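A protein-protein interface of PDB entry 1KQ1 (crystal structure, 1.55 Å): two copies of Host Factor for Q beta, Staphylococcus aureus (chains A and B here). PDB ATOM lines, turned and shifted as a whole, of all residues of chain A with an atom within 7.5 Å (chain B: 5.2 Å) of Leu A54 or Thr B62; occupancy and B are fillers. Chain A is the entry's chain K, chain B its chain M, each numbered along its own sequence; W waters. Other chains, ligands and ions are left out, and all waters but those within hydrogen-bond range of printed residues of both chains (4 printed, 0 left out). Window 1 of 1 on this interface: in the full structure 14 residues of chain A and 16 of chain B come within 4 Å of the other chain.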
ATOM      1  N   VAL A  24      -2.863 -20.429  27.024  1.00  0.00           N
ATOM      2  CA  VAL A  24      -3.952 -20.754  26.101  1.00  0.00           C
ATOM      3  C   VAL A  24      -3.615 -20.216  24.714  1.00  0.00           C
ATOM      4  O   VAL A  24      -3.334 -19.005  24.554  1.00  0.00           O
ATOM      5  CB  VAL A  24      -5.280 -20.116  26.559  1.00  0.00           C
ATOM      6  CG1 VAL A  24      -6.405 -20.392  25.544  1.00  0.00           C
ATOM      7  CG2 VAL A  24      -5.696 -20.690  27.921  1.00  0.00           C
ATOM      8  N   PHE A  26      -5.057 -19.674  20.842  1.00  0.00           N
ATOM      9  CA  PHE A  26      -6.314 -19.525  20.122  1.00  0.00           C
ATOM     10  C   PHE A  26      -6.217 -20.039  18.715  1.00  0.00           C
ATOM     11  O   PHE A  26      -5.107 -20.317  18.217  1.00  0.00           O
ATOM     12  CB  PHE A  26      -6.659 -18.023  20.113  1.00  0.00           C
ATOM     13  CG  PHE A  26      -6.912 -17.476  21.490  1.00  0.00           C
ATOM     14  CD1 PHE A  26      -8.174 -17.513  22.050  1.00  0.00           C
ATOM     15  CD2 PHE A  26      -5.859 -16.956  22.217  1.00  0.00           C
ATOM     16  CE1 PHE A  26      -8.354 -17.011  23.366  1.00  0.00           C
ATOM     17  CE2 PHE A  26      -6.050 -16.470  23.499  1.00  0.00           C
ATOM     18  CZ  PHE A  26      -7.294 -16.508  24.047  1.00  0.00           C
ATOM     19  N   MET A  32      -2.065 -16.542  25.365  1.00  0.00           N
ATOM     20  CA  MET A  32      -2.228 -15.771  26.586  1.00  0.00           C
ATOM     21  C   MET A  32      -1.895 -16.702  27.735  1.00  0.00           C
ATOM     22  O   MET A  32      -2.390 -17.817  27.813  1.00  0.00           O
ATOM     23  CB  MET A  32      -3.681 -15.321  26.699  1.00  0.00           C
ATOM     24  CG  MET A  32      -3.943 -14.345  27.754  1.00  0.00           C
ATOM     25  SD  MET A  32      -5.727 -14.190  27.746  1.00  0.00           S
ATOM     26  CE  MET A  32      -6.123 -13.700  26.043  1.00  0.00           C
ATOM     27  N   GLU A  38     -12.117 -20.328  36.597  1.00  0.00           N
ATOM     28  CA  GLU A  38     -13.416 -20.993  36.497  1.00  0.00           C
ATOM     29  C   GLU A  38     -13.535 -21.563  35.077  1.00  0.00           C
ATOM     30  O   GLU A  38     -12.818 -21.114  34.179  1.00  0.00           O
ATOM     31  CB  GLU A  38     -14.550 -19.972  36.663  1.00  0.00           C
ATOM     32  CG  GLU A  38     -14.515 -19.125  37.928  1.00  0.00           C
ATOM     33  CD  GLU A  38     -15.767 -18.260  38.073  1.00  0.00           C
ATOM     34  OE1 GLU A  38     -16.051 -17.456  37.161  1.00  0.00           O
ATOM     35  OE2 GLU A  38     -16.466 -18.381  39.100  1.00  0.00           O
ATOM     36  N   TYR A  39     -14.433 -22.517  34.884  1.00  0.00           N
ATOM     37  CA  TYR A  39     -14.674 -23.068  33.549  1.00  0.00           C
ATOM     38  C   TYR A  39     -15.949 -23.855  33.598  1.00  0.00           C
ATOM     39  O   TYR A  39     -16.443 -24.243  34.668  1.00  0.00           O
ATOM     40  CB  TYR A  39     -13.517 -23.986  33.086  1.00  0.00           C
ATOM     41  CG  TYR A  39     -13.437 -25.249  33.892  1.00  0.00           C
ATOM     42  CD1 TYR A  39     -14.117 -26.408  33.516  1.00  0.00           C
ATOM     43  CD2 TYR A  39     -12.733 -25.241  35.094  1.00  0.00           C
ATOM     44  CE1 TYR A  39     -14.096 -27.551  34.338  1.00  0.00           C
ATOM     45  CE2 TYR A  39     -12.715 -26.365  35.913  1.00  0.00           C
ATOM     46  CZ  TYR A  39     -13.383 -27.496  35.542  1.00  0.00           C
ATOM     47  OH  TYR A  39     -13.390 -28.582  36.403  1.00  0.00           O
ATOM     48  N   ASP A  40     -16.525 -24.038  32.424  1.00  0.00           N
ATOM     49  CA  ASP A  40     -17.703 -24.876  32.321  1.00  0.00           C
ATOM     50  C   ASP A  40     -17.669 -25.544  30.957  1.00  0.00           C
ATOM     51  O   ASP A  40     -16.601 -25.624  30.341  1.00  0.00           O
ATOM     52  CB  ASP A  40     -19.009 -24.139  32.620  1.00  0.00           C
ATOM     53  CG  ASP A  40     -19.372 -23.074  31.617  1.00  0.00           C
ATOM     54  OD1 ASP A  40     -18.921 -23.139  30.461  1.00  0.00           O
ATOM     55  OD2 ASP A  40     -20.170 -22.178  31.984  1.00  0.00           O
ATOM     56  N   TYR A  42     -18.630 -24.620  28.096  1.00  0.00           N
ATOM     57  CA  TYR A  42     -18.369 -23.788  26.947  1.00  0.00           C
ATOM     58  C   TYR A  42     -17.339 -22.691  27.098  1.00  0.00           C
ATOM     59  O   TYR A  42     -16.852 -22.208  26.072  1.00  0.00           O
ATOM     60  CB  TYR A  42     -19.671 -23.153  26.507  1.00  0.00           C
ATOM     61  CG  TYR A  42     -20.692 -24.166  26.054  1.00  0.00           C
ATOM     62  CD1 TYR A  42     -20.526 -24.848  24.858  1.00  0.00           C
ATOM     63  CD2 TYR A  42     -21.797 -24.459  26.837  1.00  0.00           C
ATOM     64  CE1 TYR A  42     -21.446 -25.809  24.440  1.00  0.00           C
ATOM     65  CE2 TYR A  42     -22.719 -25.415  26.438  1.00  0.00           C
ATOM     66  CZ  TYR A  42     -22.538 -26.086  25.241  1.00  0.00           C
ATOM     67  OH  TYR A  42     -23.447 -27.048  24.855  1.00  0.00           O
ATOM     68  N   VAL A  43     -16.979 -22.311  28.329  1.00  0.00           N
ATOM     69  CA  VAL A  43     -16.037 -21.204  28.507  1.00  0.00           C
ATOM     70  C   VAL A  43     -15.014 -21.499  29.599  1.00  0.00           C
ATOM     71  O   VAL A  43     -15.173 -22.415  30.405  1.00  0.00           O
ATOM     72  CB  VAL A  43     -16.746 -19.884  28.906  1.00  0.00           C
ATOM     73  CG1 VAL A  43     -17.789 -19.502  27.859  1.00  0.00           C
ATOM     74  CG2 VAL A  43     -17.434 -20.047  30.272  1.00  0.00           C
ATOM     75  N   VAL A  44     -13.946 -20.720  29.527  1.00  0.00           N
ATOM     76  CA  VAL A  44     -12.853 -20.764  30.486  1.00  0.00           C
ATOM     77  C   VAL A  44     -12.591 -19.342  30.955  1.00  0.00           C
ATOM     78  O   VAL A  44     -12.498 -18.431  30.140  1.00  0.00           O
ATOM     79  CB  VAL A  44     -11.565 -21.315  29.834  1.00  0.00           C
ATOM     80  CG1 VAL A  44     -10.374 -21.193  30.773  1.00  0.00           C
ATOM     81  CG2 VAL A  44     -11.818 -22.787  29.478  1.00  0.00           C
ATOM     82  N   SER A  45     -12.507 -19.099  32.276  1.00  0.00           N
ATOM     83  CA  SER A  45     -12.193 -17.775  32.767  1.00  0.00           C
ATOM     84  C   SER A  45     -10.713 -17.789  33.152  1.00  0.00           C
ATOM     85  O   SER A  45     -10.339 -18.529  34.078  1.00  0.00           O
ATOM     86  CB  SER A  45     -13.057 -17.452  34.003  1.00  0.00           C
ATOM     87  OG  SER A  45     -12.702 -16.167  34.495  1.00  0.00           O
ATOM     88  N   LEU A  46      -9.914 -16.974  32.455  1.00  0.00           N
ATOM     89  CA  LEU A  46      -8.472 -16.935  32.619  1.00  0.00           C
ATOM     90  C   LEU A  46      -8.010 -15.582  33.157  1.00  0.00           C
ATOM     91  O   LEU A  46      -8.323 -14.541  32.602  1.00  0.00           O
ATOM     92  CB  LEU A  46      -7.785 -17.180  31.247  1.00  0.00           C
ATOM     93  CG  LEU A  46      -6.260 -17.273  31.283  1.00  0.00           C
ATOM     94  CD1 LEU A  46      -5.807 -18.628  31.794  1.00  0.00           C
ATOM     95  CD2 LEU A  46      -5.701 -17.082  29.838  1.00  0.00           C
ATOM     96  N   ASN A  47      -7.272 -15.588  34.264  1.00  0.00           N
ATOM     97  CA  ASN A  47      -6.734 -14.346  34.824  1.00  0.00           C
ATOM     98  C   ASN A  47      -5.294 -14.201  34.279  1.00  0.00           C
ATOM     99  O   ASN A  47      -4.470 -15.097  34.472  1.00  0.00           O
ATOM    100  CB  ASN A  47      -6.755 -14.471  36.347  1.00  0.00           C
ATOM    101  CG  ASN A  47      -6.308 -13.200  37.037  1.00  0.00           C
ATOM    102  OD1 ASN A  47      -5.174 -12.771  36.884  1.00  0.00           O
ATOM    103  ND2 ASN A  47      -7.210 -12.588  37.796  1.00  0.00           N
ATOM    104  N   LYS A  51      -5.735  -8.431  33.655  1.00  0.00           N
ATOM    105  CA  LYS A  51      -6.949  -8.618  32.868  1.00  0.00           C
ATOM    106  C   LYS A  51      -7.655  -9.953  33.159  1.00  0.00           C
ATOM    107  O   LYS A  51      -7.026 -10.977  33.439  1.00  0.00           O
ATOM    108  CB  LYS A  51      -6.628  -8.591  31.369  1.00  0.00           C
ATOM    109  CG  LYS A  51      -6.159  -7.254  30.807  1.00  0.00           C
ATOM    110  CD  LYS A  51      -7.298  -6.255  30.676  1.00  0.00           C
ATOM    111  CE  LYS A  51      -8.358  -6.662  29.647  1.00  0.00           C
ATOM    112  NZ  LYS A  51      -9.309  -5.536  29.303  1.00  0.00           N
ATOM    113  N   GLN A  52      -8.980  -9.934  33.117  1.00  0.00           N
ATOM    114  CA  GLN A  52      -9.745 -11.172  33.291  1.00  0.00           C
ATOM    115  C   GLN A  52     -10.244 -11.439  31.890  1.00  0.00           C
ATOM    116  O   GLN A  52     -10.724 -10.520  31.228  1.00  0.00           O
ATOM    117  CB  GLN A  52     -10.957 -10.975  34.205  1.00  0.00           C
ATOM    118  CG  GLN A  52     -11.603 -12.294  34.627  1.00  0.00           C
ATOM    119  CD  GLN A  52     -10.650 -13.140  35.439  1.00  0.00           C
ATOM    120  OE1 GLN A  52      -9.756 -12.608  36.107  1.00  0.00           O
ATOM    121  NE2 GLN A  52     -10.837 -14.461  35.404  1.00  0.00           N
ATOM    122  N   HIS A  53     -10.150 -12.697  31.450  1.00  0.00           N
ATOM    123  CA  HIS A  53     -10.578 -13.066  30.102  1.00  0.00           C
ATOM    124  C   HIS A  53     -11.587 -14.196  30.159  1.00  0.00           C
ATOM    125  O   HIS A  53     -11.293 -15.278  30.704  1.00  0.00           O
ATOM    126  CB  HIS A  53      -9.389 -13.555  29.283  1.00  0.00           C
ATOM    127  CG  HIS A  53      -8.233 -12.623  29.301  1.00  0.00           C
ATOM    128  ND1 HIS A  53      -8.002 -11.687  28.314  1.00  0.00           N
ATOM    129  CD2 HIS A  53      -7.210 -12.501  30.184  1.00  0.00           C
ATOM    130  CE1 HIS A  53      -6.878 -11.041  28.573  1.00  0.00           C
ATOM    131  NE2 HIS A  53      -6.379 -11.512  29.704  1.00  0.00           N
ATOM    132  N   LEU A  54     -12.777 -13.970  29.615  1.00  0.00           N
ATOM    133  CA  LEU A  54     -13.785 -15.031  29.564  1.00  0.00           C
ATOM    134  C   LEU A  54     -13.609 -15.553  28.124  1.00  0.00           C
ATOM    135  O   LEU A  54     -13.946 -14.880  27.171  1.00  0.00           O
ATOM    136  CB  LEU A  54     -15.179 -14.450  29.783  1.00  0.00           C
ATOM    137  CG  LEU A  54     -16.242 -15.523  29.710  1.00  0.00           C
ATOM    138  CD1 LEU A  54     -15.964 -16.577  30.794  1.00  0.00           C
ATOM    139  CD2 LEU A  54     -17.616 -14.877  29.886  1.00  0.00           C
ATOM    140  N   ILE A  55     -13.119 -16.772  28.002  1.00  0.00           N
ATOM    141  CA  ILE A  55     -12.770 -17.330  26.693  1.00  0.00           C
ATOM    142  C   ILE A  55     -13.707 -18.431  26.250  1.00  0.00           C
ATOM    143  O   ILE A  55     -13.982 -19.360  27.002  1.00  0.00           O
ATOM    144  CB  ILE A  55     -11.350 -17.956  26.777  1.00  0.00           C
ATOM    145  CG1 ILE A  55     -10.321 -16.917  27.222  1.00  0.00           C
ATOM    146  CG2 ILE A  55     -10.999 -18.607  25.433  1.00  0.00           C
ATOM    147  CD1 ILE A  55      -8.893 -17.511  27.609  1.00  0.00           C
ATOM    148  N   TYR A  56     -14.171 -18.388  24.995  1.00  0.00           N
ATOM    149  CA  TYR A  56     -14.984 -19.509  24.537  1.00  0.00           C
ATOM    150  C   TYR A  56     -14.065 -20.681  24.113  1.00  0.00           C
ATOM    151  O   TYR A  56     -13.058 -20.488  23.423  1.00  0.00           O
ATOM    152  CB  TYR A  56     -15.792 -19.119  23.299  1.00  0.00           C
ATOM    153  CG  TYR A  56     -17.011 -18.336  23.586  1.00  0.00           C
ATOM    154  CD1 TYR A  56     -18.089 -18.913  24.242  1.00  0.00           C
ATOM    155  CD2 TYR A  56     -17.087 -17.010  23.232  1.00  0.00           C
ATOM    156  CE1 TYR A  56     -19.224 -18.144  24.545  1.00  0.00           C
ATOM    157  CE2 TYR A  56     -18.210 -16.237  23.521  1.00  0.00           C
ATOM    158  CZ  TYR A  56     -19.278 -16.809  24.192  1.00  0.00           C
ATOM    159  OH  TYR A  56     -20.348 -16.001  24.586  1.00  0.00           O
ATOM    160  N   LYS A  57     -14.399 -21.886  24.575  1.00  0.00           N
ATOM    161  CA  LYS A  57     -13.640 -23.052  24.172  1.00  0.00           C
ATOM    162  C   LYS A  57     -13.621 -23.216  22.644  1.00  0.00           C
ATOM    163  O   LYS A  57     -12.631 -23.720  22.090  1.00  0.00           O
ATOM    164  CB  LYS A  57     -14.198 -24.318  24.803  1.00  0.00           C
ATOM    165  CG  LYS A  57     -13.881 -24.374  26.312  1.00  0.00           C
ATOM    166  CD  LYS A  57     -14.486 -25.640  26.832  1.00  0.00           C
ATOM    167  CE  LYS A  57     -14.130 -25.864  28.280  1.00  0.00           C
ATOM    168  NZ  LYS A  57     -14.843 -27.116  28.730  1.00  0.00           N
ATOM    169  N   HIS A  58     -14.688 -22.763  21.983  1.00  0.00           N
ATOM    170  CA  HIS A  58     -14.657 -22.873  20.528  1.00  0.00           C
ATOM    171  C   HIS A  58     -13.527 -22.114  19.861  1.00  0.00           C
ATOM    172  O   HIS A  58     -13.188 -22.407  18.681  1.00  0.00           O
ATOM    173  CB  HIS A  58     -16.012 -22.491  19.899  1.00  0.00           C
ATOM    174  CG  HIS A  58     -16.449 -21.058  20.073  1.00  0.00           C
ATOM    175  ND1 HIS A  58     -17.718 -20.751  20.514  1.00  0.00           N
ATOM    176  CD2 HIS A  58     -15.871 -19.873  19.751  1.00  0.00           C
ATOM    177  CE1 HIS A  58     -17.909 -19.444  20.460  1.00  0.00           C
ATOM    178  NE2 HIS A  58     -16.803 -18.884  19.994  1.00  0.00           N
ATOM    179  N   ALA A  59     -12.954 -21.140  20.582  1.00  0.00           N
ATOM    180  CA  ALA A  59     -11.850 -20.366  20.043  1.00  0.00           C
ATOM    181  C   ALA A  59     -10.477 -20.838  20.501  1.00  0.00           C
ATOM    182  O   ALA A  59      -9.430 -20.241  20.102  1.00  0.00           O
ATOM    183  CB  ALA A  59     -12.069 -18.897  20.445  1.00  0.00           C
ATOM    184  N   ILE A  60     -10.466 -21.851  21.379  1.00  0.00           N
ATOM    185  CA  ILE A  60      -9.199 -22.363  21.879  1.00  0.00           C
ATOM    186  C   ILE A  60      -8.637 -23.460  21.014  1.00  0.00           C
ATOM    187  O   ILE A  60      -9.393 -24.324  20.550  1.00  0.00           O
ATOM    188  CB  ILE A  60      -9.352 -22.851  23.347  1.00  0.00           C
ATOM    189  CG1 ILE A  60      -9.805 -21.685  24.208  1.00  0.00           C
ATOM    190  CG2 ILE A  60      -8.079 -23.525  23.813  1.00  0.00           C
ATOM    191  CD1 ILE A  60     -10.020 -22.132  25.709  1.00  0.00           C
ATOM    192  N   ILE B   7     -21.377 -19.763  34.190  1.00  0.00           N
ATOM    193  CA  ILE B   7     -20.303 -18.786  34.118  1.00  0.00           C
ATOM    194  C   ILE B   7     -20.497 -17.694  33.079  1.00  0.00           C
ATOM    195  O   ILE B   7     -20.297 -16.505  33.340  1.00  0.00           O
ATOM    196  CB  ILE B   7     -18.933 -19.471  33.814  1.00  0.00           C
ATOM    197  CG1 ILE B   7     -18.632 -20.552  34.850  1.00  0.00           C
ATOM    198  CG2 ILE B   7     -17.822 -18.424  33.768  1.00  0.00           C
ATOM    199  CD1 ILE B   7     -18.612 -20.083  36.289  1.00  0.00           C
ATOM    200  N   GLN B   8     -20.879 -18.098  31.876  1.00  0.00           N
ATOM    201  CA  GLN B   8     -21.046 -17.136  30.824  1.00  0.00           C
ATOM    202  C   GLN B   8     -22.157 -16.119  31.060  1.00  0.00           C
ATOM    203  O   GLN B   8     -21.973 -14.906  30.918  1.00  0.00           O
ATOM    204  CB  GLN B   8     -21.242 -17.912  29.494  1.00  0.00           C
ATOM    205  CG  GLN B   8     -21.659 -17.052  28.389  1.00  0.00           C
ATOM    206  CD  GLN B   8     -21.898 -17.781  27.065  1.00  0.00           C
ATOM    207  OE1 GLN B   8     -22.122 -17.122  26.079  1.00  0.00           O
ATOM    208  NE2 GLN B   8     -21.836 -19.115  27.050  1.00  0.00           N
ATOM    209  N   ALA B  11     -21.400 -13.684  33.880  1.00  0.00           N
ATOM    210  CA  ALA B  11     -20.488 -12.633  33.490  1.00  0.00           C
ATOM    211  C   ALA B  11     -21.177 -11.588  32.646  1.00  0.00           C
ATOM    212  O   ALA B  11     -21.021 -10.405  32.869  1.00  0.00           O
ATOM    213  CB  ALA B  11     -19.301 -13.251  32.696  1.00  0.00           C
ATOM    214  N   LEU B  12     -21.905 -12.028  31.614  1.00  0.00           N
ATOM    215  CA  LEU B  12     -22.579 -11.069  30.761  1.00  0.00           C
ATOM    216  C   LEU B  12     -23.633 -10.253  31.509  1.00  0.00           C
ATOM    217  O   LEU B  12     -23.860  -9.096  31.188  1.00  0.00           O
ATOM    218  CB  LEU B  12     -23.207 -11.762  29.548  1.00  0.00           C
ATOM    219  CG  LEU B  12     -22.235 -12.058  28.380  1.00  0.00           C
ATOM    220  CD1 LEU B  12     -20.853 -12.513  28.841  1.00  0.00           C
ATOM    221  CD2 LEU B  12     -22.884 -13.114  27.517  1.00  0.00           C
ATOM    222  N   PHE B  15     -21.637  -7.612  33.301  1.00  0.00           N
ATOM    223  CA  PHE B  15     -21.193  -6.586  32.377  1.00  0.00           C
ATOM    224  C   PHE B  15     -22.351  -5.639  31.979  1.00  0.00           C
ATOM    225  O   PHE B  15     -22.168  -4.440  31.905  1.00  0.00           O
ATOM    226  CB  PHE B  15     -20.687  -7.218  31.066  1.00  0.00           C
ATOM    227  CG  PHE B  15     -19.447  -8.100  31.212  1.00  0.00           C
ATOM    228  CD1 PHE B  15     -18.558  -7.945  32.264  1.00  0.00           C
ATOM    229  CD2 PHE B  15     -19.204  -9.088  30.257  1.00  0.00           C
ATOM    230  CE1 PHE B  15     -17.418  -8.780  32.366  1.00  0.00           C
ATOM    231  CE2 PHE B  15     -18.060  -9.932  30.349  1.00  0.00           C
ATOM    232  CZ  PHE B  15     -17.189  -9.760  31.404  1.00  0.00           C
ATOM    233  N   THR B  23     -13.891  -5.473  26.229  1.00  0.00           N
ATOM    234  CA  THR B  23     -13.207  -5.557  24.941  1.00  0.00           C
ATOM    235  C   THR B  23     -13.517  -6.947  24.431  1.00  0.00           C
ATOM    236  O   THR B  23     -13.205  -7.941  25.104  1.00  0.00           O
ATOM    237  CB  THR B  23     -11.696  -5.384  25.065  1.00  0.00           C
ATOM    238  OG1 THR B  23     -11.416  -4.070  25.579  1.00  0.00           O
ATOM    239  CG2 THR B  23     -11.022  -5.512  23.706  1.00  0.00           C
ATOM    240  N   VAL B  24     -14.167  -7.013  23.270  1.00  0.00           N
ATOM    241  CA  VAL B  24     -14.522  -8.302  22.652  1.00  0.00           C
ATOM    242  C   VAL B  24     -13.456  -8.616  21.615  1.00  0.00           C
ATOM    243  O   VAL B  24     -13.178  -7.778  20.752  1.00  0.00           O
ATOM    244  CB  VAL B  24     -15.894  -8.227  21.953  1.00  0.00           C
ATOM    245  CG1 VAL B  24     -16.174  -9.560  21.212  1.00  0.00           C
ATOM    246  CG2 VAL B  24     -16.988  -7.976  22.964  1.00  0.00           C
ATOM    247  N   PHE B  25     -12.815  -9.776  21.750  1.00  0.00           N
ATOM    248  CA  PHE B  25     -11.839 -10.232  20.757  1.00  0.00           C
ATOM    249  C   PHE B  25     -12.578 -11.241  19.884  1.00  0.00           C
ATOM    250  O   PHE B  25     -13.355 -12.087  20.379  1.00  0.00           O
ATOM    251  CB  PHE B  25     -10.645 -10.908  21.407  1.00  0.00           C
ATOM    252  CG  PHE B  25      -9.679  -9.931  21.985  1.00  0.00           C
ATOM    253  CD1 PHE B  25      -8.548  -9.583  21.268  1.00  0.00           C
ATOM    254  CD2 PHE B  25      -9.945  -9.290  23.187  1.00  0.00           C
ATOM    255  CE1 PHE B  25      -7.679  -8.601  21.728  1.00  0.00           C
ATOM    256  CE2 PHE B  25      -9.066  -8.287  23.665  1.00  0.00           C
ATOM    257  CZ  PHE B  25      -7.939  -7.954  22.924  1.00  0.00           C
ATOM    258  N   ILE B  60     -16.921 -14.834  18.484  1.00  0.00           N
ATOM    259  CA  ILE B  60     -16.163 -14.277  19.595  1.00  0.00           C
ATOM    260  C   ILE B  60     -15.148 -15.263  20.147  1.00  0.00           C
ATOM    261  O   ILE B  60     -15.412 -16.470  20.260  1.00  0.00           O
ATOM    262  CB  ILE B  60     -17.147 -13.876  20.725  1.00  0.00           C
ATOM    263  CG1 ILE B  60     -18.059 -12.734  20.202  1.00  0.00           C
ATOM    264  CG2 ILE B  60     -16.362 -13.465  22.032  1.00  0.00           C
ATOM    265  CD1 ILE B  60     -19.177 -12.343  21.218  1.00  0.00           C
ATOM    266  N   SER B  61     -13.961 -14.748  20.454  1.00  0.00           N
ATOM    267  CA  SER B  61     -12.934 -15.578  21.126  1.00  0.00           C
ATOM    268  C   SER B  61     -12.919 -15.288  22.624  1.00  0.00           C
ATOM    269  O   SER B  61     -12.960 -16.234  23.436  1.00  0.00           O
ATOM    270  CB  SER B  61     -11.547 -15.359  20.539  1.00  0.00           C
ATOM    271  OG  SER B  61     -11.170 -14.012  20.587  1.00  0.00           O
ATOM    272  N   THR B  62     -12.885 -14.022  23.007  1.00  0.00           N
ATOM    273  CA  THR B  62     -12.822 -13.657  24.430  1.00  0.00           C
ATOM    274  C   THR B  62     -13.526 -12.362  24.749  1.00  0.00           C
ATOM    275  O   THR B  62     -13.637 -11.472  23.896  1.00  0.00           O
ATOM    276  CB  THR B  62     -11.341 -13.439  24.834  1.00  0.00           C
ATOM    277  OG1 THR B  62     -10.553 -14.529  24.373  1.00  0.00           O
ATOM    278  CG2 THR B  62     -11.165 -13.365  26.317  1.00  0.00           C
ATOM    279  N   TYR B  63     -14.013 -12.260  25.988  1.00  0.00           N
ATOM    280  CA  TYR B  63     -14.507 -10.999  26.504  1.00  0.00           C
ATOM    281  C   TYR B  63     -13.425 -10.631  27.500  1.00  0.00           C
ATOM    282  O   TYR B  63     -13.112 -11.420  28.393  1.00  0.00           O
ATOM    283  CB  TYR B  63     -15.809 -11.145  27.290  1.00  0.00           C
ATOM    284  CG  TYR B  63     -16.936 -11.682  26.509  1.00  0.00           C
ATOM    285  CD1 TYR B  63     -17.803 -10.842  25.771  1.00  0.00           C
ATOM    286  CD2 TYR B  63     -17.172 -13.032  26.502  1.00  0.00           C
ATOM    287  CE1 TYR B  63     -18.871 -11.371  25.072  1.00  0.00           C
ATOM    288  CE2 TYR B  63     -18.226 -13.587  25.805  1.00  0.00           C
ATOM    289  CZ  TYR B  63     -19.091 -12.743  25.093  1.00  0.00           C
ATOM    290  OH  TYR B  63     -20.166 -13.321  24.486  1.00  0.00           O
ATOM    291  N   THR B  64     -12.846  -9.438  27.393  1.00  0.00           N
ATOM    292  CA  THR B  64     -11.805  -9.091  28.335  1.00  0.00           C
ATOM    293  C   THR B  64     -12.166  -7.786  29.019  1.00  0.00           C
ATOM    294  O   THR B  64     -12.742  -6.847  28.430  1.00  0.00           O
ATOM    295  CB  THR B  64     -10.440  -8.956  27.611  1.00  0.00           C
ATOM    296  OG1 THR B  64     -10.485  -7.846  26.710  1.00  0.00           O
ATOM    297  CG2 THR B  64     -10.120 -10.234  26.831  1.00  0.00           C
HETATM  298  O   HOH W   1      -8.072  -5.716  26.547  1.00  0.00           O
HETATM  299  O   HOH W   2     -21.172 -20.886  30.144  1.00  0.00           O
HETATM  300  O   HOH W   3     -14.008 -11.162  31.443  1.00  0.00           O
HETATM  301  O   HOH W   4     -21.323 -22.834  34.724  1.00  0.00           O
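OD2 of Asp A40 lies within hydrogen-bond range of N of Ile B7, at 3.5 Å.
The backbone carbonyl oxygen (O) of Tyr B63 sits at hydrogen-bond distance from the backbone NH (N) of Leu A54.
OH of Tyr A56 sits at hydrogen-bond distance from OE1 of Gln B8 (2.6 Å).
O of Ser B61 is in hydrogen-bond range of N of Tyr A56, 2.9 Å away.
OH of Tyr A56 is in hydrogen-bond range of OH of Tyr B63 (2.7 Å).
O of Ile B60 lies within hydrogen-bond range of NE2 of His A58 (2.8 Å).
The side-chain sulfur of Met A32 sits close to a ring nitrogen (NE2) of His A53, at 3.4 Å.
O of Glu A38 lies within hydrogen-bond range of N of Ser A45 (2.8 Å).
The side-chain carboxylate (OD1) of Asp A40 is in hydrogen-bond range of the backbone NH (N) of Val A43.
The backbone NH of Leu A46 lies within hydrogen-bond range of the backbone carbonyl oxygen of His A53, at 2.8 Å.
The side-chain amide nitrogen (ND2) of Asn A47 lies within hydrogen-bond range of the side-chain amide oxygen (OE1) of Gln A52 (3.1 Å).
The backbone NH of Phe B25 lies within hydrogen-bond range of the backbone carbonyl oxygen of Thr B62, 2.9 Å away.
Phe A26 touches Thr B62.
OE1 of Glu A38 touches CD1 of Ile B7 (3.8 Å).
Val A43 touches Ile B7.
Lys A51 touches Thr B64 (NZ to C, 3.6 Å).
Tyr B63 touches Gln A52 (O to O, 3.8 Å).
CB of His A53 touches CG2 of Thr B62, at 3.5 Å.
Thr B64 touches His A53.
O of Leu A54 touches CA of Thr B62, 3.2 Å away.
Ile B60 touches Tyr A56 (O to CD2, 3.5 Å).
Ala A59 touches Ser B61.
Of the printed residues of chain B, Val A43 touches Ile B7 (3.9 Å).
Printed residues of chain B within 4 Å of Gln A52: Tyr B63 and Thr B64.
Leu A54 touches just these residues of chain B: Ile B7 (3.96 Å), Ala B11 (3.7 Å), Thr B62 (3.2 Å) and Tyr B63 (2.8 Å).
Of chain A, only Ile A55, Tyr A56 and Ala A59 come within 4 Å of Ser B61.
Of chain A, only Phe A26 (3.5 Å), His A53 (3.5 Å), Leu A54 (3.2 Å) and Ile A55 (3.7 Å) come within 4 Å of Thr B62.
The nearest residue of chain B that does not touch Leu A54 is Ser B61 (4.1 Å).
Hydrophobic or aromatic side chains of chain A that line the printed part of chain B: Phe A26, Val A43, His A53, Leu A54, Ile A55, Tyr A56, His A58 and Ala A59.
Of the 13 printed residues of chain B, 8 touch a printed residue of chain A.
Printed residues of chain B that touch a printed residue of chain A: Ile B7, Gln B8, Ala B11, Ile B60, Ser B61, Thr B62, Tyr B63 and Thr B64.
Hydrophobic or aromatic side chains of chain B within 4 Å of the printed part of chain A: Ile B7, Ala B11, Ile B60 and Tyr B63.
Positions printed for both chains: 24 and 60.
Water W2 lies within hydrogen-bond range of OD2 of Asp A40 (2.5 Å) and N of Gln B8 (3.3 Å).
Water W1 bridges NZ of Lys A51 and OG1 of Thr B64.
Water W4 lies within hydrogen-bond range of the side-chain carboxylate (OD2) of Asp A40 (3.0 Å) and the backbone NH (N) of Ile B7 (3.1 Å).
Water W3 lies within hydrogen-bond range of the backbone carbonyl oxygen of Tyr B63 (3.2 Å) and the backbone carbonyl oxygen of Gln A52 (3.4 Å).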
